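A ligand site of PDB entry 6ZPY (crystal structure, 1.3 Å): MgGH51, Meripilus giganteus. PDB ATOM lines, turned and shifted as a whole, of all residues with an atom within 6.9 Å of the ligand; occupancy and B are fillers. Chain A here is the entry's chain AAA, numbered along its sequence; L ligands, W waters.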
ATOM      1  N   MET A  21       8.727  -2.205 -18.578  1.00  0.00           N
ATOM      2  CA  MET A  21       8.958  -3.261 -19.586  1.00  0.00           C
ATOM      3  C   MET A  21       8.450  -4.587 -19.070  1.00  0.00           C
ATOM      4  O   MET A  21       8.926  -5.037 -18.021  1.00  0.00           O
ATOM      5  CB  MET A  21      10.447  -3.350 -19.909  1.00  0.00           C
ATOM      6  CG  MET A  21      10.766  -4.365 -20.994  1.00  0.00           C
ATOM      7  SD  MET A  21      10.948  -5.995 -20.420  1.00  0.00           S
ATOM      8  CE  MET A  21      11.253  -6.910 -21.913  1.00  0.00           C
ATOM      9  N   GLU A  23       7.421  -8.679 -19.986  1.00  0.00           N
ATOM     10  CA  GLU A  23       7.202  -9.947 -20.672  1.00  0.00           C
ATOM     11  C   GLU A  23       6.928 -10.951 -19.554  1.00  0.00           C
ATOM     12  O   GLU A  23       7.322 -10.679 -18.411  1.00  0.00           O
ATOM     13  CB  GLU A  23       8.375 -10.411 -21.503  1.00  0.00           C
ATOM     14  CG  GLU A  23       9.545 -10.846 -20.690  1.00  0.00           C
ATOM     15  CD  GLU A  23      10.802 -11.170 -21.476  1.00  0.00           C
ATOM     16  OE1 GLU A  23      10.738 -12.051 -22.335  1.00  0.00           O
ATOM     17  OE2 GLU A  23      11.791 -10.547 -21.228  1.00  0.00           O
ATOM     18  N   ILE A  25       8.357 -13.520 -17.749  1.00  0.00           N
ATOM     19  CA  ILE A  25       9.683 -14.027 -17.383  1.00  0.00           C
ATOM     20  C   ILE A  25       9.622 -14.144 -15.859  1.00  0.00           C
ATOM     21  O   ILE A  25       8.967 -13.314 -15.223  1.00  0.00           O
ATOM     22  CB  ILE A  25      10.811 -13.098 -17.861  1.00  0.00           C
ATOM     23  CG1 ILE A  25      12.181 -13.676 -17.561  1.00  0.00           C
ATOM     24  CG2 ILE A  25      10.658 -11.701 -17.290  1.00  0.00           C
ATOM     25  CD1 ILE A  25      13.317 -12.847 -18.086  1.00  0.00           C
ATOM     26  N   ARG A 226       5.661  -1.409 -22.080  1.00  0.00           N
ATOM     27  CA  ARG A 226       6.162  -2.113 -23.275  1.00  0.00           C
ATOM     28  C   ARG A 226       5.818  -3.582 -23.103  1.00  0.00           C
ATOM     29  O   ARG A 226       6.129  -4.160 -22.059  1.00  0.00           O
ATOM     30  CB  ARG A 226       7.680  -1.931 -23.330  1.00  0.00           C
ATOM     31  CG  ARG A 226       8.348  -2.487 -24.581  1.00  0.00           C
ATOM     32  CD  ARG A 226       9.857  -2.737 -24.337  1.00  0.00           C
ATOM     33  NE  ARG A 226      10.411  -3.401 -25.492  1.00  0.00           N
ATOM     34  CZ  ARG A 226      11.411  -4.246 -25.444  1.00  0.00           C
ATOM     35  NH1 ARG A 226      12.112  -4.402 -24.331  1.00  0.00           N
ATOM     36  NH2 ARG A 226      11.760  -4.877 -26.544  1.00  0.00           N
ATOM     37  N   GLY A 229       6.928  -8.423 -25.131  1.00  0.00           N
ATOM     38  CA  GLY A 229       8.343  -8.790 -24.982  1.00  0.00           C
ATOM     39  C   GLY A 229       9.228  -7.972 -25.910  1.00  0.00           C
ATOM     40  O   GLY A 229       8.667  -7.252 -26.731  1.00  0.00           O
ATOM     41  N   GLY A 230      10.539  -8.043 -25.732  1.00  0.00           N
ATOM     42  CA  GLY A 230      11.176  -9.089 -24.956  1.00  0.00           C
ATOM     43  C   GLY A 230      11.227 -10.425 -25.669  1.00  0.00           C
ATOM     44  O   GLY A 230      10.486 -10.671 -26.618  1.00  0.00           O
ATOM     45  N   ASN A 231      12.067 -11.309 -25.157  1.00  0.00           N
ATOM     46  CA  ASN A 231      12.224 -12.637 -25.790  1.00  0.00           C
ATOM     47  C   ASN A 231      10.905 -13.385 -25.889  1.00  0.00           C
ATOM     48  O   ASN A 231      10.732 -14.141 -26.807  1.00  0.00           O
ATOM     49  CB  ASN A 231      13.234 -13.445 -25.021  1.00  0.00           C
ATOM     50  CG  ASN A 231      14.652 -13.088 -25.362  1.00  0.00           C
ATOM     51  OD1 ASN A 231      14.919 -12.088 -26.019  1.00  0.00           O
ATOM     52  ND2 ASN A 231      15.590 -13.851 -24.828  1.00  0.00           N
ATOM     53  N   ASN A 232      10.044 -13.192 -24.909  1.00  0.00           N
ATOM     54  CA  ASN A 232       8.815 -13.984 -24.857  1.00  0.00           C
ATOM     55  C   ASN A 232       7.881 -13.667 -26.017  1.00  0.00           C
ATOM     56  O   ASN A 232       6.962 -14.415 -26.266  1.00  0.00           O
ATOM     57  CB  ASN A 232       8.040 -13.781 -23.561  1.00  0.00           C
ATOM     58  CG  ASN A 232       7.249 -15.024 -23.148  1.00  0.00           C
ATOM     59  OD1 ASN A 232       7.812 -16.139 -23.131  1.00  0.00           O
ATOM     60  ND2 ASN A 232       5.982 -14.814 -22.851  1.00  0.00           N
ATOM     61  N   GLU A 234       9.091 -13.642 -29.100  1.00  0.00           N
ATOM     62  CA  GLU A 234       9.718 -14.181 -30.297  1.00  0.00           C
ATOM     63  C   GLU A 234       9.407 -15.650 -30.521  1.00  0.00           C
ATOM     64  O   GLU A 234       9.349 -16.047 -31.667  1.00  0.00           O
ATOM     65  CB  GLU A 234      11.197 -13.918 -30.265  1.00  0.00           C
ATOM     66  CG  GLU A 234      11.539 -12.455 -30.428  1.00  0.00           C
ATOM     67  CD  GLU A 234      12.996 -12.180 -30.241  1.00  0.00           C
ATOM     68  OE1 GLU A 234      13.747 -12.160 -31.266  1.00  0.00           O
ATOM     69  OE2 GLU A 234      13.406 -11.949 -29.125  1.00  0.00           O
ATOM     70  N   TRP A 261      11.065 -18.875 -21.595  1.00  0.00           N
ATOM     71  CA  TRP A 261      11.779 -18.915 -20.294  1.00  0.00           C
ATOM     72  C   TRP A 261      11.551 -20.226 -19.553  1.00  0.00           C
ATOM     73  O   TRP A 261      11.729 -20.260 -18.330  1.00  0.00           O
ATOM     74  CB  TRP A 261      11.360 -17.690 -19.493  1.00  0.00           C
ATOM     75  CG  TRP A 261      11.813 -16.425 -20.142  1.00  0.00           C
ATOM     76  CD1 TRP A 261      11.017 -15.548 -20.812  1.00  0.00           C
ATOM     77  CD2 TRP A 261      13.160 -15.978 -20.294  1.00  0.00           C
ATOM     78  NE1 TRP A 261      11.817 -14.523 -21.281  1.00  0.00           N
ATOM     79  CE2 TRP A 261      13.113 -14.740 -20.948  1.00  0.00           C
ATOM     80  CE3 TRP A 261      14.380 -16.433 -19.812  1.00  0.00           C
ATOM     81  CZ2 TRP A 261      14.255 -13.993 -21.216  1.00  0.00           C
ATOM     82  CZ3 TRP A 261      15.507 -15.681 -20.055  1.00  0.00           C
ATOM     83  CH2 TRP A 261      15.451 -14.488 -20.769  1.00  0.00           C
ATOM     84  N   ASN A 350      11.885  -7.876 -31.499  1.00  0.00           N
ATOM     85  CA  ASN A 350      12.672  -7.683 -30.289  1.00  0.00           C
ATOM     86  C   ASN A 350      14.128  -8.029 -30.568  1.00  0.00           C
ATOM     87  O   ASN A 350      14.400  -9.117 -31.100  1.00  0.00           O
ATOM     88  CB  ASN A 350      12.169  -8.652 -29.196  1.00  0.00           C
ATOM     89  CG  ASN A 350      12.940  -8.489 -27.911  1.00  0.00           C
ATOM     90  OD1 ASN A 350      12.928  -7.408 -27.300  1.00  0.00           O
ATOM     91  ND2 ASN A 350      13.656  -9.541 -27.499  1.00  0.00           N
ATOM     92  N   GLU A 351      15.035  -7.140 -30.206  1.00  0.00           N
ATOM     93  CA  GLU A 351      16.487  -7.437 -30.274  1.00  0.00           C
ATOM     94  C   GLU A 351      16.797  -8.057 -31.626  1.00  0.00           C
ATOM     95  O   GLU A 351      17.492  -9.048 -31.691  1.00  0.00           O
ATOM     96  CB  GLU A 351      16.916  -8.298 -29.083  1.00  0.00           C
ATOM     97  CG  GLU A 351      16.783  -7.530 -27.785  1.00  0.00           C
ATOM     98  CD  GLU A 351      17.584  -8.110 -26.644  1.00  0.00           C
ATOM     99  OE1 GLU A 351      17.907  -9.305 -26.752  1.00  0.00           O
ATOM    100  OE2 GLU A 351      17.914  -7.335 -25.740  1.00  0.00           O
ATOM    101  N   PHE A 353      19.009  -6.988 -33.534  1.00  0.00           N
ATOM    102  CA  PHE A 353      20.469  -6.988 -33.761  1.00  0.00           C
ATOM    103  C   PHE A 353      20.957  -8.438 -33.893  1.00  0.00           C
ATOM    104  O   PHE A 353      21.932  -8.699 -34.595  1.00  0.00           O
ATOM    105  CB  PHE A 353      21.189  -6.159 -32.718  1.00  0.00           C
ATOM    106  CG  PHE A 353      20.825  -6.446 -31.272  1.00  0.00           C
ATOM    107  CD1 PHE A 353      21.382  -7.519 -30.597  1.00  0.00           C
ATOM    108  CD2 PHE A 353      19.950  -5.624 -30.616  1.00  0.00           C
ATOM    109  CE1 PHE A 353      21.114  -7.706 -29.259  1.00  0.00           C
ATOM    110  CE2 PHE A 353      19.624  -5.868 -29.295  1.00  0.00           C
ATOM    111  CZ  PHE A 353      20.232  -6.886 -28.618  1.00  0.00           C
ATOM    112  N   PHE A 354      20.309  -9.402 -33.219  1.00  0.00           N
ATOM    113  CA  PHE A 354      20.720 -10.809 -33.324  1.00  0.00           C
ATOM    114  C   PHE A 354      20.381 -11.393 -34.695  1.00  0.00           C
ATOM    115  O   PHE A 354      20.887 -12.454 -35.029  1.00  0.00           O
ATOM    116  CB  PHE A 354      20.036 -11.626 -32.236  1.00  0.00           C
ATOM    117  CG  PHE A 354      20.665 -11.507 -30.864  1.00  0.00           C
ATOM    118  CD1 PHE A 354      22.007 -11.746 -30.649  1.00  0.00           C
ATOM    119  CD2 PHE A 354      19.902 -11.054 -29.798  1.00  0.00           C
ATOM    120  CE1 PHE A 354      22.557 -11.648 -29.385  1.00  0.00           C
ATOM    121  CE2 PHE A 354      20.440 -10.998 -28.529  1.00  0.00           C
ATOM    122  CZ  PHE A 354      21.772 -11.309 -28.319  1.00  0.00           C
ATOM    123  N   HIS A 400      18.939  -1.281 -25.682  1.00  0.00           N
ATOM    124  CA  HIS A 400      19.004  -2.091 -24.460  1.00  0.00           C
ATOM    125  C   HIS A 400      20.440  -2.137 -23.958  1.00  0.00           C
ATOM    126  O   HIS A 400      21.355  -2.325 -24.759  1.00  0.00           O
ATOM    127  CB  HIS A 400      18.601  -3.541 -24.729  1.00  0.00           C
ATOM    128  CG  HIS A 400      17.235  -3.722 -25.242  1.00  0.00           C
ATOM    129  ND1 HIS A 400      16.727  -4.950 -25.674  1.00  0.00           N
ATOM    130  CD2 HIS A 400      16.247  -2.832 -25.442  1.00  0.00           C
ATOM    131  CE1 HIS A 400      15.490  -4.786 -26.095  1.00  0.00           C
ATOM    132  NE2 HIS A 400      15.170  -3.506 -25.949  1.00  0.00           N
ATOM    133  N   TYR A 402      22.569  -3.956 -20.494  1.00  0.00           N
ATOM    134  CA  TYR A 402      22.796  -4.641 -19.207  1.00  0.00           C
ATOM    135  C   TYR A 402      24.266  -4.521 -18.903  1.00  0.00           C
ATOM    136  O   TYR A 402      25.083  -4.917 -19.739  1.00  0.00           O
ATOM    137  CB  TYR A 402      22.320  -6.072 -19.326  1.00  0.00           C
ATOM    138  CG  TYR A 402      20.842  -6.200 -19.550  1.00  0.00           C
ATOM    139  CD1 TYR A 402      19.927  -5.953 -18.554  1.00  0.00           C
ATOM    140  CD2 TYR A 402      20.356  -6.513 -20.793  1.00  0.00           C
ATOM    141  CE1 TYR A 402      18.568  -6.127 -18.760  1.00  0.00           C
ATOM    142  CE2 TYR A 402      18.994  -6.629 -21.031  1.00  0.00           C
ATOM    143  CZ  TYR A 402      18.103  -6.471 -20.008  1.00  0.00           C
ATOM    144  OH  TYR A 402      16.784  -6.618 -20.210  1.00  0.00           O
ATOM    145  N   GLU A 429      15.126  -1.548 -22.352  1.00  0.00           N
ATOM    146  CA  GLU A 429      15.628  -2.452 -21.315  1.00  0.00           C
ATOM    147  C   GLU A 429      16.949  -1.926 -20.811  1.00  0.00           C
ATOM    148  O   GLU A 429      17.867  -1.740 -21.602  1.00  0.00           O
ATOM    149  CB  GLU A 429      15.881  -3.853 -21.878  1.00  0.00           C
ATOM    150  CG  GLU A 429      14.654  -4.537 -22.401  1.00  0.00           C
ATOM    151  CD  GLU A 429      14.902  -5.891 -23.033  1.00  0.00           C
ATOM    152  OE1 GLU A 429      15.916  -6.547 -22.655  1.00  0.00           O
ATOM    153  OE2 GLU A 429      14.095  -6.268 -23.878  1.00  0.00           O
ATOM    154  N   PHE A 441      26.603 -11.742 -17.399  1.00  0.00           N
ATOM    155  CA  PHE A 441      25.448 -12.649 -17.414  1.00  0.00           C
ATOM    156  C   PHE A 441      25.761 -13.950 -16.671  1.00  0.00           C
ATOM    157  O   PHE A 441      25.080 -14.943 -16.945  1.00  0.00           O
ATOM    158  CB  PHE A 441      24.995 -12.858 -18.851  1.00  0.00           C
ATOM    159  CG  PHE A 441      24.705 -11.575 -19.565  1.00  0.00           C
ATOM    160  CD1 PHE A 441      23.520 -10.907 -19.380  1.00  0.00           C
ATOM    161  CD2 PHE A 441      25.629 -11.047 -20.457  1.00  0.00           C
ATOM    162  CE1 PHE A 441      23.271  -9.734 -20.051  1.00  0.00           C
ATOM    163  CE2 PHE A 441      25.375  -9.855 -21.103  1.00  0.00           C
ATOM    164  CZ  PHE A 441      24.199  -9.201 -20.914  1.00  0.00           C
ATOM    165  N   ALA A 480      14.599  -3.426 -16.946  1.00  0.00           N
ATOM    166  CA  ALA A 480      14.131  -4.791 -17.192  1.00  0.00           C
ATOM    167  C   ALA A 480      15.023  -5.792 -16.502  1.00  0.00           C
ATOM    168  O   ALA A 480      16.223  -5.584 -16.409  1.00  0.00           O
ATOM    169  CB  ALA A 480      14.113  -5.091 -18.661  1.00  0.00           C
ATOM    170  N   PRO A 481      14.461  -6.969 -16.104  1.00  0.00           N
ATOM    171  CA  PRO A 481      13.029  -7.246 -16.073  1.00  0.00           C
ATOM    172  C   PRO A 481      12.312  -6.566 -14.919  1.00  0.00           C
ATOM    173  O   PRO A 481      12.930  -6.169 -13.912  1.00  0.00           O
ATOM    174  CB  PRO A 481      12.927  -8.775 -15.891  1.00  0.00           C
ATOM    175  CG  PRO A 481      14.326  -9.288 -16.204  1.00  0.00           C
ATOM    176  CD  PRO A 481      15.267  -8.170 -15.794  1.00  0.00           C
ATOM    177  N   LEU A 482      11.010  -6.473 -15.093  1.00  0.00           N
ATOM    178  CA  LEU A 482      10.167  -5.773 -14.116  1.00  0.00           C
ATOM    179  C   LEU A 482       9.883  -6.644 -12.890  1.00  0.00           C
ATOM    180  O   LEU A 482       9.872  -6.109 -11.797  1.00  0.00           O
ATOM    181  CB  LEU A 482       8.861  -5.443 -14.822  1.00  0.00           C
ATOM    182  CG  LEU A 482       7.834  -4.685 -14.032  1.00  0.00           C
ATOM    183  CD1 LEU A 482       8.357  -3.345 -13.566  1.00  0.00           C
ATOM    184  CD2 LEU A 482       6.600  -4.514 -14.901  1.00  0.00           C
ATOM    185  N   TRP A 491      16.062 -14.914 -14.463  1.00  0.00           N
ATOM    186  CA  TRP A 491      16.887 -13.701 -14.651  1.00  0.00           C
ATOM    187  C   TRP A 491      16.862 -12.878 -13.376  1.00  0.00           C
ATOM    188  O   TRP A 491      15.775 -12.679 -12.870  1.00  0.00           O
ATOM    189  CB  TRP A 491      16.376 -12.864 -15.840  1.00  0.00           C
ATOM    190  CG  TRP A 491      17.215 -11.679 -16.196  1.00  0.00           C
ATOM    191  CD1 TRP A 491      17.384 -10.552 -15.474  1.00  0.00           C
ATOM    192  CD2 TRP A 491      18.008 -11.554 -17.362  1.00  0.00           C
ATOM    193  NE1 TRP A 491      18.249  -9.716 -16.116  1.00  0.00           N
ATOM    194  CE2 TRP A 491      18.625 -10.290 -17.294  1.00  0.00           C
ATOM    195  CE3 TRP A 491      18.174 -12.345 -18.481  1.00  0.00           C
ATOM    196  CZ2 TRP A 491      19.387  -9.785 -18.341  1.00  0.00           C
ATOM    197  CZ3 TRP A 491      18.970 -11.858 -19.495  1.00  0.00           C
ATOM    198  CH2 TRP A 491      19.572 -10.611 -19.406  1.00  0.00           C
ATOM    199  N   ASP A 494      15.836  -8.058 -10.740  1.00  0.00           N
ATOM    200  CA  ASP A 494      14.498  -7.672 -11.198  1.00  0.00           C
ATOM    201  C   ASP A 494      13.955  -6.520 -10.352  1.00  0.00           C
ATOM    202  O   ASP A 494      14.325  -6.381  -9.199  1.00  0.00           O
ATOM    203  CB  ASP A 494      13.572  -8.868 -11.159  1.00  0.00           C
ATOM    204  CG  ASP A 494      14.167 -10.016 -11.914  1.00  0.00           C
ATOM    205  OD1 ASP A 494      14.074 -10.018 -13.157  1.00  0.00           O
ATOM    206  OD2 ASP A 494      14.693 -10.964 -11.230  1.00  0.00           O
HETATM  207  O1  LIG L   1      14.946  -8.676 -19.784  1.00  0.00           O
HETATM  208  C1  LIG L   1      15.387 -10.029 -20.169  1.00  0.00           C
HETATM  209  C2  LIG L   1      15.812 -10.251 -21.646  1.00  0.00           C
HETATM  210  O2  LIG L   1      16.876  -9.331 -22.019  1.00  0.00           O
HETATM  211  C3  LIG L   1      14.750  -9.886 -22.636  1.00  0.00           C
HETATM  212  O3  LIG L   1      13.726 -10.822 -22.883  1.00  0.00           O
HETATM  213  C4  LIG L   1      15.578  -9.587 -23.957  1.00  0.00           C
HETATM  214  O4  LIG L   1      14.775  -8.786 -24.835  1.00  0.00           O
HETATM  215  C5  LIG L   1      16.929  -9.047 -23.449  1.00  0.00           C
HETATM  216  O5  LIG L   1      17.853 -10.029 -24.009  1.00  0.00           O
HETATM  217  O   HOH W   1      12.163  -8.821 -19.166  1.00  0.00           O
HETATM  218  O   HOH W   2      20.304  -9.612 -22.816  1.00  0.00           O
HETATM  219  O   HOH W   3      18.337 -12.636 -23.577  1.00  0.00           O
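Water W3 bridges an oxygen (O5) of the ligand (2.7 Å) and the side-chain amide nitrogen of Asn 231 (3.3 Å).
Water W1 lies within hydrogen-bond range of the side-chain carboxylate (OE2) of Glu 23 (2.7 Å), an oxygen (O1) of the ligand (2.9 Å) and the side-chain sulfur (SD) of Met 21 (3.3 Å).
The side-chain carboxylate (OE1) of Glu 23 sits at hydrogen-bond distance from the indole nitrogen (NE1) of Trp 261 (2.9 Å).
OH of Tyr 402 lies within hydrogen-bond range of OE1 of Glu 429.
OE2 of Glu 429 sits close to ND1 of His 400 (3.4 Å).
ND1 of His 400 is in hydrogen-bond range of OE2 of Glu 351, 2.7 Å away.
The side-chain amide nitrogen of Asn 350 sits at hydrogen-bond distance from the side-chain amide oxygen of Asn 231, 3.2 Å away.
The side-chain amide oxygen (OD1) of Asn 231 lies close to the side-chain carboxylate (OE2) of Glu 234 (3.5 Å).
N of Gly 230 is in hydrogen-bond range of OD1 of Asn 350 (2.9 Å).
The side-chain amide oxygen of Asn 350 lies within hydrogen-bond range of the guanidinium group of Arg 226, at 2.9 Å.
O3 of the ligand sits at hydrogen-bond distance from OE2 of Glu 23.
O4 of the ligand is in hydrogen-bond range of OE2 of Glu 429.
The side-chain hydroxyl of Tyr 402 is in hydrogen-bond range of an oxygen (O1) of the ligand (2.8 Å).
OE1 of Glu 351 sits at hydrogen-bond distance from O5 of the ligand, at 2.8 Å.
O3 of the ligand lies within hydrogen-bond range of N of Asn 231, at 2.9 Å.
The side-chain amide nitrogen (ND2) of Asn 350 sits at hydrogen-bond distance from an oxygen (O4) of the ligand (3.0 Å).
Merely in contact with the ligand: Gly 230, Trp 261, Ala 480, Pro 481 and Trp 491.
11 residues have an atom within 4 Å of the ligand: Glu 23, Gly 230, Asn 231, Trp 261, Asn 350, Glu 351, Tyr 402, Glu 429, Ala 480, Pro 481 and Trp 491.
The nearest printed residue that does not touch the ligand is Ile 25 (4.1 Å).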
